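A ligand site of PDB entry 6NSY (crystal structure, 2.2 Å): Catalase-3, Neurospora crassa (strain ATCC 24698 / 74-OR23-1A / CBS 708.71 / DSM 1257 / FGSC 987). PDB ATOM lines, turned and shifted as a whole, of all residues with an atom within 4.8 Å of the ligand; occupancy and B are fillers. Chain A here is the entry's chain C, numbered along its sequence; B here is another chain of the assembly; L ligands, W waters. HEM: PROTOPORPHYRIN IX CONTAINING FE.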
ATOM      1  N   ARG A  99      -1.545  16.329 -28.240  1.00  0.00           N
ATOM      2  CA  ARG A  99      -1.644  16.733 -26.840  1.00  0.00           C
ATOM      3  C   ARG A  99      -0.974  15.677 -25.953  1.00  0.00           C
ATOM      4  O   ARG A  99      -1.105  14.472 -26.183  1.00  0.00           O
ATOM      5  CB  ARG A  99      -3.109  16.898 -26.436  1.00  0.00           C
ATOM      6  CG  ARG A  99      -3.842  18.068 -27.073  1.00  0.00           C
ATOM      7  CD  ARG A  99      -5.362  17.811 -27.026  1.00  0.00           C
ATOM      8  NE  ARG A  99      -6.156  18.950 -27.467  1.00  0.00           N
ATOM      9  CZ  ARG A  99      -6.256  19.358 -28.732  1.00  0.00           C
ATOM     10  NH1 ARG A  99      -5.615  18.728 -29.712  1.00  0.00           N
ATOM     11  NH2 ARG A  99      -6.999  20.423 -29.011  1.00  0.00           N
ATOM     12  N   VAL A 100      -0.272  16.151 -24.918  1.00  0.00           N
ATOM     13  CA  VAL A 100       0.488  15.221 -24.072  1.00  0.00           C
ATOM     14  C   VAL A 100      -0.443  14.275 -23.325  1.00  0.00           C
ATOM     15  O   VAL A 100      -0.107  13.106 -23.086  1.00  0.00           O
ATOM     16  CB  VAL A 100       1.427  15.992 -23.127  1.00  0.00           C
ATOM     17  CG1 VAL A 100       0.632  16.695 -22.026  1.00  0.00           C
ATOM     18  CG2 VAL A 100       2.473  15.068 -22.530  1.00  0.00           C
ATOM     19  N   VAL A 101      -1.632  14.745 -22.938  1.00  0.00           N
ATOM     20  CA  VAL A 101      -2.722  13.903 -22.492  1.00  0.00           C
ATOM     21  C   VAL A 101      -3.969  14.352 -23.229  1.00  0.00           C
ATOM     22  O   VAL A 101      -4.021  15.459 -23.776  1.00  0.00           O
ATOM     23  CB  VAL A 101      -2.959  13.953 -20.959  1.00  0.00           C
ATOM     24  CG1 VAL A 101      -1.844  13.219 -20.217  1.00  0.00           C
ATOM     25  CG2 VAL A 101      -3.074  15.392 -20.477  1.00  0.00           C
ATOM     26  N   HIS A 102      -4.977  13.479 -23.242  1.00  0.00           N
ATOM     27  CA  HIS A 102      -6.237  13.729 -23.955  1.00  0.00           C
ATOM     28  C   HIS A 102      -6.017  13.890 -25.464  1.00  0.00           C
ATOM     29  O   HIS A 102      -6.701  14.676 -26.117  1.00  0.00           O
ATOM     30  CB  HIS A 102      -6.960  14.960 -23.416  1.00  0.00           C
ATOM     31  CG  HIS A 102      -7.440  14.840 -22.001  1.00  0.00           C
ATOM     32  ND1 HIS A 102      -8.763  14.648 -21.673  1.00  0.00           N
ATOM     33  CD2 HIS A 102      -6.778  14.917 -20.823  1.00  0.00           C
ATOM     34  CE1 HIS A 102      -8.903  14.607 -20.360  1.00  0.00           C
ATOM     35  NE2 HIS A 102      -7.701  14.763 -19.818  1.00  0.00           N
ATOM     36  N   ARG A 139     -14.556  20.418 -26.418  1.00  0.00           N
ATOM     37  CA  ARG A 139     -13.806  19.272 -26.911  1.00  0.00           C
ATOM     38  C   ARG A 139     -13.906  18.173 -25.861  1.00  0.00           C
ATOM     39  O   ARG A 139     -13.588  18.393 -24.688  1.00  0.00           O
ATOM     40  CB  ARG A 139     -12.343  19.622 -27.186  1.00  0.00           C
ATOM     41  CG  ARG A 139     -11.529  18.498 -27.820  1.00  0.00           C
ATOM     42  CD  ARG A 139     -10.106  18.937 -28.224  1.00  0.00           C
ATOM     43  NE  ARG A 139      -9.334  17.855 -28.821  1.00  0.00           N
ATOM     44  CZ  ARG A 139      -8.721  16.893 -28.124  1.00  0.00           C
ATOM     45  NH1 ARG A 139      -8.781  16.901 -26.797  1.00  0.00           N
ATOM     46  NH2 ARG A 139      -8.049  15.927 -28.741  1.00  0.00           N
ATOM     47  N   SER A 141     -12.876  14.002 -24.984  1.00  0.00           N
ATOM     48  CA  SER A 141     -11.665  13.230 -25.229  1.00  0.00           C
ATOM     49  C   SER A 141     -11.582  12.041 -24.286  1.00  0.00           C
ATOM     50  O   SER A 141     -12.322  11.954 -23.300  1.00  0.00           O
ATOM     51  CB  SER A 141     -10.417  14.114 -25.049  1.00  0.00           C
ATOM     52  OG  SER A 141     -10.481  14.841 -23.828  1.00  0.00           O
ATOM     53  N   GLY A 158     -12.302  13.677 -21.036  1.00  0.00           N
ATOM     54  CA  GLY A 158     -12.261  15.112 -20.961  1.00  0.00           C
ATOM     55  C   GLY A 158     -13.580  15.724 -21.396  1.00  0.00           C
ATOM     56  O   GLY A 158     -14.318  15.171 -22.210  1.00  0.00           O
ATOM     57  N   PHE A 159     -13.869  16.887 -20.816  1.00  0.00           N
ATOM     58  CA  PHE A 159     -15.090  17.654 -21.108  1.00  0.00           C
ATOM     59  C   PHE A 159     -14.687  19.111 -20.913  1.00  0.00           C
ATOM     60  O   PHE A 159     -14.825  19.659 -19.818  1.00  0.00           O
ATOM     61  CB  PHE A 159     -16.231  17.218 -20.198  1.00  0.00           C
ATOM     62  CG  PHE A 159     -17.602  17.792 -20.554  1.00  0.00           C
ATOM     63  CD1 PHE A 159     -17.742  19.026 -21.177  1.00  0.00           C
ATOM     64  CD2 PHE A 159     -18.751  17.085 -20.216  1.00  0.00           C
ATOM     65  CE1 PHE A 159     -18.997  19.534 -21.477  1.00  0.00           C
ATOM     66  CE2 PHE A 159     -20.023  17.593 -20.517  1.00  0.00           C
ATOM     67  CZ  PHE A 159     -20.152  18.815 -21.150  1.00  0.00           C
ATOM     68  N   ALA A 160     -14.160  19.720 -21.979  1.00  0.00           N
ATOM     69  CA  ALA A 160     -13.521  21.028 -21.915  1.00  0.00           C
ATOM     70  C   ALA A 160     -14.342  22.060 -22.700  1.00  0.00           C
ATOM     71  O   ALA A 160     -14.603  21.857 -23.886  1.00  0.00           O
ATOM     72  CB  ALA A 160     -12.102  20.962 -22.466  1.00  0.00           C
ATOM     73  N   VAL A 173     -12.026  23.577 -17.912  1.00  0.00           N
ATOM     74  CA  VAL A 173     -11.299  22.427 -18.464  1.00  0.00           C
ATOM     75  C   VAL A 173     -11.580  21.258 -17.521  1.00  0.00           C
ATOM     76  O   VAL A 173     -10.873  21.035 -16.538  1.00  0.00           O
ATOM     77  CB  VAL A 173      -9.807  22.724 -18.608  1.00  0.00           C
ATOM     78  CG1 VAL A 173      -9.118  21.571 -19.332  1.00  0.00           C
ATOM     79  CG2 VAL A 173      -9.607  24.037 -19.370  1.00  0.00           C
ATOM     80  N   GLY A 174     -12.632  20.507 -17.840  1.00  0.00           N
ATOM     81  CA  GLY A 174     -13.160  19.512 -16.940  1.00  0.00           C
ATOM     82  C   GLY A 174     -13.090  18.094 -17.497  1.00  0.00           C
ATOM     83  O   GLY A 174     -12.624  17.853 -18.608  1.00  0.00           O
ATOM     84  N   ASN A 175     -13.600  17.160 -16.685  1.00  0.00           N
ATOM     85  CA  ASN A 175     -13.685  15.751 -17.009  1.00  0.00           C
ATOM     86  C   ASN A 175     -15.110  15.272 -16.771  1.00  0.00           C
ATOM     87  O   ASN A 175     -15.937  15.981 -16.189  1.00  0.00           O
ATOM     88  CB  ASN A 175     -12.696  14.909 -16.172  1.00  0.00           C
ATOM     89  CG  ASN A 175     -11.290  14.925 -16.737  1.00  0.00           C
ATOM     90  OD1 ASN A 175     -11.073  15.269 -17.891  1.00  0.00           O
ATOM     91  ND2 ASN A 175     -10.318  14.555 -15.893  1.00  0.00           N
ATOM     92  N   PHE A 180     -10.208  13.575  -9.216  1.00  0.00           N
ATOM     93  CA  PHE A 180      -8.999  13.221  -9.942  1.00  0.00           C
ATOM     94  C   PHE A 180      -8.107  12.319  -9.109  1.00  0.00           C
ATOM     95  O   PHE A 180      -8.255  12.216  -7.887  1.00  0.00           O
ATOM     96  CB  PHE A 180      -8.224  14.466 -10.391  1.00  0.00           C
ATOM     97  CG  PHE A 180      -7.352  14.215 -11.579  1.00  0.00           C
ATOM     98  CD1 PHE A 180      -7.916  13.874 -12.798  1.00  0.00           C
ATOM     99  CD2 PHE A 180      -5.968  14.251 -11.471  1.00  0.00           C
ATOM    100  CE1 PHE A 180      -7.131  13.611 -13.902  1.00  0.00           C
ATOM    101  CE2 PHE A 180      -5.173  13.994 -12.569  1.00  0.00           C
ATOM    102  CZ  PHE A 180      -5.748  13.675 -13.788  1.00  0.00           C
ATOM    103  N   ALA A 185      -0.105  18.600  -8.073  1.00  0.00           N
ATOM    104  CA  ALA A 185       0.169  18.632  -9.507  1.00  0.00           C
ATOM    105  C   ALA A 185       1.572  18.137  -9.851  1.00  0.00           C
ATOM    106  O   ALA A 185       1.795  17.684 -10.976  1.00  0.00           O
ATOM    107  CB  ALA A 185      -0.023  20.044 -10.050  1.00  0.00           C
ATOM    108  N   PHE A 188       1.555  14.582 -11.439  1.00  0.00           N
ATOM    109  CA  PHE A 188       0.905  14.249 -12.707  1.00  0.00           C
ATOM    110  C   PHE A 188       1.786  13.465 -13.674  1.00  0.00           C
ATOM    111  O   PHE A 188       1.280  12.495 -14.279  1.00  0.00           O
ATOM    112  CB  PHE A 188       0.394  15.546 -13.368  1.00  0.00           C
ATOM    113  CG  PHE A 188      -0.595  15.317 -14.478  1.00  0.00           C
ATOM    114  CD1 PHE A 188      -1.853  14.820 -14.201  1.00  0.00           C
ATOM    115  CD2 PHE A 188      -0.283  15.644 -15.788  1.00  0.00           C
ATOM    116  CE1 PHE A 188      -2.780  14.618 -15.214  1.00  0.00           C
ATOM    117  CE2 PHE A 188      -1.223  15.449 -16.805  1.00  0.00           C
ATOM    118  CZ  PHE A 188      -2.463  14.934 -16.505  1.00  0.00           C
ATOM    119  N   GLY A 247     -16.008  20.489 -13.248  1.00  0.00           N
ATOM    120  CA  GLY A 247     -14.744  21.213 -13.133  1.00  0.00           C
ATOM    121  C   GLY A 247     -13.767  20.557 -12.181  1.00  0.00           C
ATOM    122  O   GLY A 247     -12.566  20.873 -12.241  1.00  0.00           O
ATOM    123  N   ILE A 248     -14.244  19.651 -11.326  1.00  0.00           N
ATOM    124  CA  ILE A 248     -13.491  18.925 -10.303  1.00  0.00           C
ATOM    125  C   ILE A 248     -13.090  19.853  -9.163  1.00  0.00           C
ATOM    126  O   ILE A 248     -13.612  19.739  -8.051  1.00  0.00           O
ATOM    127  CB  ILE A 248     -12.270  18.199 -10.893  1.00  0.00           C
ATOM    128  CG1 ILE A 248     -12.723  17.191 -11.963  1.00  0.00           C
ATOM    129  CG2 ILE A 248     -11.502  17.491  -9.779  1.00  0.00           C
ATOM    130  CD1 ILE A 248     -11.792  16.009 -12.132  1.00  0.00           C
ATOM    131  N   HIS A 249     -12.160  20.770  -9.421  1.00  0.00           N
ATOM    132  CA  HIS A 249     -11.676  21.659  -8.370  1.00  0.00           C
ATOM    133  C   HIS A 249     -12.773  22.581  -7.845  1.00  0.00           C
ATOM    134  O   HIS A 249     -13.707  22.963  -8.566  1.00  0.00           O
ATOM    135  CB  HIS A 249     -10.528  22.533  -8.863  1.00  0.00           C
ATOM    136  CG  HIS A 249      -9.443  21.786  -9.583  1.00  0.00           C
ATOM    137  ND1 HIS A 249      -8.578  20.933  -8.933  1.00  0.00           N
ATOM    138  CD2 HIS A 249      -9.095  21.768 -10.893  1.00  0.00           C
ATOM    139  CE1 HIS A 249      -7.745  20.413  -9.820  1.00  0.00           C
ATOM    140  NE2 HIS A 249      -8.033  20.903 -11.013  1.00  0.00           N
ATOM    141  N   ILE A 363      -7.155  23.977 -30.981  1.00  0.00           N
ATOM    142  CA  ILE A 363      -7.646  24.763 -29.856  1.00  0.00           C
ATOM    143  C   ILE A 363      -6.819  24.446 -28.628  1.00  0.00           C
ATOM    144  O   ILE A 363      -6.369  23.309 -28.428  1.00  0.00           O
ATOM    145  CB  ILE A 363      -9.152  24.557 -29.624  1.00  0.00           C
ATOM    146  CG1 ILE A 363      -9.676  25.641 -28.671  1.00  0.00           C
ATOM    147  CG2 ILE A 363      -9.446  23.153 -29.072  1.00  0.00           C
ATOM    148  CD1 ILE A 363     -11.157  25.544 -28.364  1.00  0.00           C
ATOM    149  N   SER A 364      -6.566  25.466 -27.800  1.00  0.00           N
ATOM    150  CA  SER A 364      -5.616  25.391 -26.691  1.00  0.00           C
ATOM    151  C   SER A 364      -6.320  25.800 -25.396  1.00  0.00           C
ATOM    152  O   SER A 364      -6.421  26.991 -25.091  1.00  0.00           O
ATOM    153  CB  SER A 364      -4.402  26.280 -26.955  1.00  0.00           C
ATOM    154  OG  SER A 364      -3.566  25.723 -27.949  1.00  0.00           O
ATOM    155  N   PHE A 365      -6.787  24.814 -24.648  1.00  0.00           N
ATOM    156  CA  PHE A 365      -7.481  25.073 -23.398  1.00  0.00           C
ATOM    157  C   PHE A 365      -6.488  25.365 -22.280  1.00  0.00           C
ATOM    158  O   PHE A 365      -5.350  24.877 -22.288  1.00  0.00           O
ATOM    159  CB  PHE A 365      -8.367  23.887 -23.009  1.00  0.00           C
ATOM    160  CG  PHE A 365      -9.629  23.802 -23.816  1.00  0.00           C
ATOM    161  CD1 PHE A 365     -10.704  24.637 -23.545  1.00  0.00           C
ATOM    162  CD2 PHE A 365      -9.749  22.883 -24.856  1.00  0.00           C
ATOM    163  CE1 PHE A 365     -11.875  24.547 -24.281  1.00  0.00           C
ATOM    164  CE2 PHE A 365     -10.920  22.794 -25.592  1.00  0.00           C
ATOM    165  CZ  PHE A 365     -11.984  23.640 -25.302  1.00  0.00           C
ATOM    166  N   LEU A 381      -3.612  20.670  -6.913  1.00  0.00           N
ATOM    167  CA  LEU A 381      -3.637  20.117  -8.264  1.00  0.00           C
ATOM    168  C   LEU A 381      -3.948  21.219  -9.272  1.00  0.00           C
ATOM    169  O   LEU A 381      -3.266  21.348 -10.296  1.00  0.00           O
ATOM    170  CB  LEU A 381      -4.667  18.996  -8.342  1.00  0.00           C
ATOM    171  CG  LEU A 381      -4.646  18.071  -9.556  1.00  0.00           C
ATOM    172  CD1 LEU A 381      -3.420  17.193  -9.473  1.00  0.00           C
ATOM    173  CD2 LEU A 381      -5.908  17.227  -9.570  1.00  0.00           C
ATOM    174  N   GLY A 384      -0.819  23.767  -9.998  1.00  0.00           N
ATOM    175  CA  GLY A 384       0.162  23.405 -11.011  1.00  0.00           C
ATOM    176  C   GLY A 384      -0.376  23.340 -12.422  1.00  0.00           C
ATOM    177  O   GLY A 384       0.379  23.529 -13.375  1.00  0.00           O
ATOM    178  N   ARG A 385      -1.679  23.077 -12.577  1.00  0.00           N
ATOM    179  CA  ARG A 385      -2.283  23.088 -13.904  1.00  0.00           C
ATOM    180  C   ARG A 385      -2.096  24.436 -14.589  1.00  0.00           C
ATOM    181  O   ARG A 385      -1.786  24.495 -15.784  1.00  0.00           O
ATOM    182  CB  ARG A 385      -3.773  22.745 -13.819  1.00  0.00           C
ATOM    183  CG  ARG A 385      -4.066  21.268 -13.563  1.00  0.00           C
ATOM    184  CD  ARG A 385      -5.551  21.040 -13.510  1.00  0.00           C
ATOM    185  NE  ARG A 385      -6.153  20.898 -14.829  1.00  0.00           N
ATOM    186  CZ  ARG A 385      -7.426  21.176 -15.096  1.00  0.00           C
ATOM    187  NH1 ARG A 385      -8.202  21.663 -14.144  1.00  0.00           N
ATOM    188  NH2 ARG A 385      -7.901  21.012 -16.322  1.00  0.00           N
ATOM    189  N   SER A 388       1.122  24.417 -16.261  1.00  0.00           N
ATOM    190  CA  SER A 388       1.380  23.361 -17.245  1.00  0.00           C
ATOM    191  C   SER A 388       0.712  23.645 -18.577  1.00  0.00           C
ATOM    192  O   SER A 388       1.260  23.337 -19.634  1.00  0.00           O
ATOM    193  CB  SER A 388       0.929  22.013 -16.671  1.00  0.00           C
ATOM    194  OG  SER A 388       0.932  21.000 -17.653  1.00  0.00           O
ATOM    195  N   TYR A 389      -0.497  24.214 -18.554  1.00  0.00           N
ATOM    196  CA  TYR A 389      -1.246  24.393 -19.799  1.00  0.00           C
ATOM    197  C   TYR A 389      -0.699  25.534 -20.637  1.00  0.00           C
ATOM    198  O   TYR A 389      -0.726  25.455 -21.867  1.00  0.00           O
ATOM    199  CB  TYR A 389      -2.717  24.661 -19.521  1.00  0.00           C
ATOM    200  CG  TYR A 389      -3.488  23.475 -19.039  1.00  0.00           C
ATOM    201  CD1 TYR A 389      -3.180  22.878 -17.817  1.00  0.00           C
ATOM    202  CD2 TYR A 389      -4.558  22.969 -19.772  1.00  0.00           C
ATOM    203  CE1 TYR A 389      -3.902  21.818 -17.348  1.00  0.00           C
ATOM    204  CE2 TYR A 389      -5.291  21.902 -19.308  1.00  0.00           C
ATOM    205  CZ  TYR A 389      -4.949  21.344 -18.091  1.00  0.00           C
ATOM    206  OH  TYR A 389      -5.672  20.311 -17.616  1.00  0.00           O
ATOM    207  N   THR A 392       2.699  24.072 -22.047  1.00  0.00           N
ATOM    208  CA  THR A 392       2.616  22.992 -23.030  1.00  0.00           C
ATOM    209  C   THR A 392       2.203  23.495 -24.418  1.00  0.00           C
ATOM    210  O   THR A 392       2.487  22.814 -25.403  1.00  0.00           O
ATOM    211  CB  THR A 392       1.642  21.892 -22.576  1.00  0.00           C
ATOM    212  OG1 THR A 392       1.928  20.685 -23.298  1.00  0.00           O
ATOM    213  CG2 THR A 392       0.192  22.301 -22.831  1.00  0.00           C
ATOM    214  N   GLN A 393       1.554  24.657 -24.511  1.00  0.00           N
ATOM    215  CA  GLN A 393       1.226  25.198 -25.827  1.00  0.00           C
ATOM    216  C   GLN A 393       2.476  25.575 -26.602  1.00  0.00           C
ATOM    217  O   GLN A 393       2.472  25.555 -27.837  1.00  0.00           O
ATOM    218  CB  GLN A 393       0.290  26.405 -25.711  1.00  0.00           C
ATOM    219  CG  GLN A 393      -0.919  26.188 -24.825  1.00  0.00           C
ATOM    220  CD  GLN A 393      -1.776  25.018 -25.256  1.00  0.00           C
ATOM    221  OE1 GLN A 393      -1.808  24.663 -26.444  1.00  0.00           O
ATOM    222  NE2 GLN A 393      -2.480  24.411 -24.300  1.00  0.00           N
ATOM    223  N   ARG A 396       3.247  22.318 -28.395  1.00  0.00           N
ATOM    224  CA  ARG A 396       2.295  21.882 -29.395  1.00  0.00           C
ATOM    225  C   ARG A 396       2.209  22.875 -30.555  1.00  0.00           C
ATOM    226  O   ARG A 396       1.986  22.466 -31.706  1.00  0.00           O
ATOM    227  CB  ARG A 396       0.928  21.663 -28.745  1.00  0.00           C
ATOM    228  CG  ARG A 396       0.090  20.604 -29.416  1.00  0.00           C
ATOM    229  CD  ARG A 396      -0.903  19.952 -28.450  1.00  0.00           C
ATOM    230  NE  ARG A 396      -1.845  20.915 -27.890  1.00  0.00           N
ATOM    231  CZ  ARG A 396      -2.876  21.435 -28.557  1.00  0.00           C
ATOM    232  NH1 ARG A 396      -3.684  22.282 -27.939  1.00  0.00           N
ATOM    233  NH2 ARG A 396      -3.104  21.106 -29.825  1.00  0.00           N
ATOM    234  N   LEU B  88       7.794  19.507 -14.501  1.00  0.00           N
ATOM    235  CA  LEU B  88       6.597  19.581 -15.338  1.00  0.00           C
ATOM    236  C   LEU B  88       6.911  20.124 -16.723  1.00  0.00           C
ATOM    237  O   LEU B  88       6.258  19.726 -17.693  1.00  0.00           O
ATOM    238  CB  LEU B  88       5.517  20.425 -14.666  1.00  0.00           C
ATOM    239  CG  LEU B  88       4.438  19.652 -13.907  1.00  0.00           C
ATOM    240  CD1 LEU B  88       3.593  18.812 -14.856  1.00  0.00           C
ATOM    241  CD2 LEU B  88       5.049  18.766 -12.825  1.00  0.00           C
ATOM    242  N   PHE B  91       7.835  17.167 -18.855  1.00  0.00           N
ATOM    243  CA  PHE B  91       6.639  16.387 -19.189  1.00  0.00           C
ATOM    244  C   PHE B  91       5.776  17.135 -20.192  1.00  0.00           C
ATOM    245  O   PHE B  91       5.244  16.533 -21.133  1.00  0.00           O
ATOM    246  CB  PHE B  91       5.826  16.058 -17.934  1.00  0.00           C
ATOM    247  CG  PHE B  91       4.426  15.575 -18.233  1.00  0.00           C
ATOM    248  CD1 PHE B  91       4.183  14.232 -18.471  1.00  0.00           C
ATOM    249  CD2 PHE B  91       3.350  16.449 -18.274  1.00  0.00           C
ATOM    250  CE1 PHE B  91       2.910  13.765 -18.757  1.00  0.00           C
ATOM    251  CE2 PHE B  91       2.065  16.003 -18.560  1.00  0.00           C
ATOM    252  CZ  PHE B  91       1.845  14.654 -18.803  1.00  0.00           C
ATOM    253  N   ASP B  92       5.628  18.449 -20.005  1.00  0.00           N
ATOM    254  CA  ASP B  92       4.791  19.237 -20.909  1.00  0.00           C
ATOM    255  C   ASP B  92       5.305  19.175 -22.342  1.00  0.00           C
ATOM    256  O   ASP B  92       4.517  19.366 -23.286  1.00  0.00           O
ATOM    257  CB  ASP B  92       4.734  20.698 -20.464  1.00  0.00           C
ATOM    258  CG  ASP B  92       3.983  20.902 -19.159  1.00  0.00           C
ATOM    259  OD1 ASP B  92       3.223  20.007 -18.733  1.00  0.00           O
ATOM    260  OD2 ASP B  92       4.134  21.985 -18.557  1.00  0.00           O
HETATM  261  CHA HEM L   1      -5.199  18.350 -21.194  1.00  0.00           C
HETATM  262  CHB HEM L   1      -8.641  17.945 -17.772  1.00  0.00           C
HETATM  263  CHC HEM L   1      -5.176  17.557 -14.411  1.00  0.00           C
HETATM  264  CHD HEM L   1      -1.854  18.870 -17.699  1.00  0.00           C
HETATM  265  C1A HEM L   1      -6.441  18.235 -20.576  1.00  0.00           C
HETATM  266  C2A HEM L   1      -7.730  18.192 -21.233  1.00  0.00           C
HETATM  267  C3A HEM L   1      -8.666  18.079 -20.287  1.00  0.00           C
HETATM  268  C4A HEM L   1      -8.014  18.047 -18.998  1.00  0.00           C
HETATM  269  CMA HEM L   1     -10.179  17.996 -20.547  1.00  0.00           C
HETATM  270  CAA HEM L   1      -7.987  18.257 -22.758  1.00  0.00           C
HETATM  271  CBA HEM L   1      -8.290  19.668 -23.236  1.00  0.00           C
HETATM  272  CGA HEM L   1      -8.584  19.585 -24.710  1.00  0.00           C
HETATM  273  O1A HEM L   1      -7.824  20.192 -25.508  1.00  0.00           O
HETATM  274  O2A HEM L   1      -9.568  18.892 -25.092  1.00  0.00           O
HETATM  275  C1B HEM L   1      -8.022  17.853 -16.544  1.00  0.00           C
HETATM  276  C2B HEM L   1      -8.658  17.836 -15.236  1.00  0.00           C
HETATM  277  C3B HEM L   1      -7.687  17.710 -14.310  1.00  0.00           C
HETATM  278  C4B HEM L   1      -6.417  17.668 -15.000  1.00  0.00           C
HETATM  279  CMB HEM L   1     -10.188  17.930 -15.033  1.00  0.00           C
HETATM  280  CAB HEM L   1      -7.778  17.660 -12.762  1.00  0.00           C
HETATM  281  CBB HEM L   1      -8.875  17.988 -12.069  1.00  0.00           C
HETATM  282  C1C HEM L   1      -3.987  17.956 -14.978  1.00  0.00           C
HETATM  283  C2C HEM L   1      -2.744  18.236 -14.284  1.00  0.00           C
HETATM  284  C3C HEM L   1      -1.815  18.581 -15.197  1.00  0.00           C
HETATM  285  C4C HEM L   1      -2.459  18.564 -16.500  1.00  0.00           C
HETATM  286  CMC HEM L   1      -2.579  18.101 -12.744  1.00  0.00           C
HETATM  287  CAC HEM L   1      -0.337  19.003 -14.988  1.00  0.00           C
HETATM  288  CBC HEM L   1       0.095  19.597 -13.866  1.00  0.00           C
HETATM  289  C1D HEM L   1      -2.471  18.851 -18.948  1.00  0.00           C
HETATM  290  C2D HEM L   1      -1.854  19.190 -20.211  1.00  0.00           C
HETATM  291  C3D HEM L   1      -2.778  19.051 -21.179  1.00  0.00           C
HETATM  292  C4D HEM L   1      -4.019  18.618 -20.556  1.00  0.00           C
HETATM  293  CMD HEM L   1      -0.395  19.642 -20.379  1.00  0.00           C
HETATM  294  CAD HEM L   1      -2.543  19.319 -22.680  1.00  0.00           C
HETATM  295  CBD HEM L   1      -3.175  20.675 -23.035  1.00  0.00           C
HETATM  296  CGD HEM L   1      -2.880  21.025 -24.465  1.00  0.00           C
HETATM  297  O1D HEM L   1      -3.585  21.912 -25.012  1.00  0.00           O
HETATM  298  O2D HEM L   1      -1.945  20.428 -25.054  1.00  0.00           O
HETATM  299  NA  HEM L   1      -6.656  18.147 -19.218  1.00  0.00           N
HETATM  300  NB  HEM L   1      -6.659  17.752 -16.359  1.00  0.00           N
HETATM  301  NC  HEM L   1      -3.764  18.167 -16.332  1.00  0.00           N
HETATM  302  ND  HEM L   1      -3.788  18.504 -19.195  1.00  0.00           N
HETATM  303 FE   HEM L   1      -5.216  18.177 -17.767  1.00  0.00          FE
HETATM  304  O   HOH W   1     -11.398  17.328 -23.846  1.00  0.00           O
HETATM  305  O   HOH W   2      -6.165  22.060 -24.963  1.00  0.00           O
HETATM  306  O   HOH W   3       0.319  19.021 -24.817  1.00  0.00           O
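O of Val 173 lies within hydrogen-bond range of NH2 of Arg 385 (3.0 Å). A ring nitrogen (ND1) of His 102 sits at hydrogen-bond distance from the side-chain hydroxyl (OG) of Ser 141, at 2.8 Å. NH1 of Arg 139 lies within hydrogen-bond range of O of His 102 (3.1 Å). O of Ala 160 sits at hydrogen-bond distance from N of Arg 139, at 2.9 Å. NH1 of Arg 396 is in hydrogen-bond range of OG of Ser 364 (3.4 Å). The guanidinium group (NH1) of Arg 396 sits at hydrogen-bond distance from the backbone carbonyl oxygen (O) of Ile 363. NH2 of Arg 99 is in hydrogen-bond range of O of Ile 363, at 3.0 Å. The guanidinium group (NH1) of Arg 396 is in hydrogen-bond range of the side-chain amide oxygen (OE1) of Gln 393.
Water W2 bridges O1A of the ligand (2.6 Å) and N of Phe 365 (2.8 Å). Water W3 lies within hydrogen-bond range of O2D of the ligand (2.7 Å), OG1 of Thr 392 (2.8 Å) and N of Val 100 (2.9 Å). Water W1 lies within hydrogen-bond range of the backbone carbonyl oxygen (O) of Arg 139 (2.6 Å), the side-chain hydroxyl (OG) of Ser 141 (2.7 Å) and an oxygen (O2A) of the ligand (2.7 Å).
The side-chain hydroxyl (OH) of Tyr 389 binds an iron atom (FE) of the ligand (2.2 Å). NE2 of Gln 393 is in hydrogen-bond range of O1D of the ligand. The guanidinium group of Arg 396 is in salt-bridge range of an oxygen (O2D) of the ligand, at 2.9 Å. NE of Arg 99 lies within salt-bridge range of O1A of the ligand, 2.9 Å away. The guanidinium group of Arg 139 lies within salt-bridge range of an oxygen (O2A) of the ligand (2.7 Å).
The guanidinium group of Arg 385 lies close to a nitrogen (NB) of the ligand (3.5 Å). CG1 of Val 100 touches CMD of the ligand (3.5 Å). Val 101 touches the ligand. CD2 of His 102 touches C1A of the ligand, at 3.3 Å. Gly 158 touches the ligand (CA to CMA, 3.6 Å). Phe 159 touches the ligand (N to CMA, 3.9 Å). Val 173 touches the ligand (O to CMB, 3.5 Å). Gly 174 touches the ligand (O to CMA, 3.1 Å). Asn 175 touches the ligand. Phe 180 touches the ligand (CG to CAB, 3.7 Å). Ala 185 touches the ligand (CB to CBC, 3.8 Å). Phe 188 touches the ligand. CG2 of Ile 248 touches CBB of the ligand (3.5 Å). His 249 touches the ligand. Phe 365 touches the ligand (CD2 to O1A, 3.4 Å). Leu 381 touches the ligand. Gly 384 touches the ligand (O to CBC, 3.97 Å). Ser 388 touches the ligand (OG to CMD, 3.3 Å). Thr 392 touches the ligand (CG2 to O2D, 3.6 Å). Leu 88 of chain B touches the ligand (CD1 to CBC, 3.7 Å). Asp 92 of chain B touches the ligand. Hydrophobic or aromatic side chains within 4 Å of the ligand: Val 100, Val 101, His 102, Val 173, Phe 180, Ala 185, Phe 188, Ile 248, His 249, Phe 365, Leu 381, Tyr 389 and Leu 88 of chain B. Along chain A the residues within 4 Å of the ligand span positions 99 to 396.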
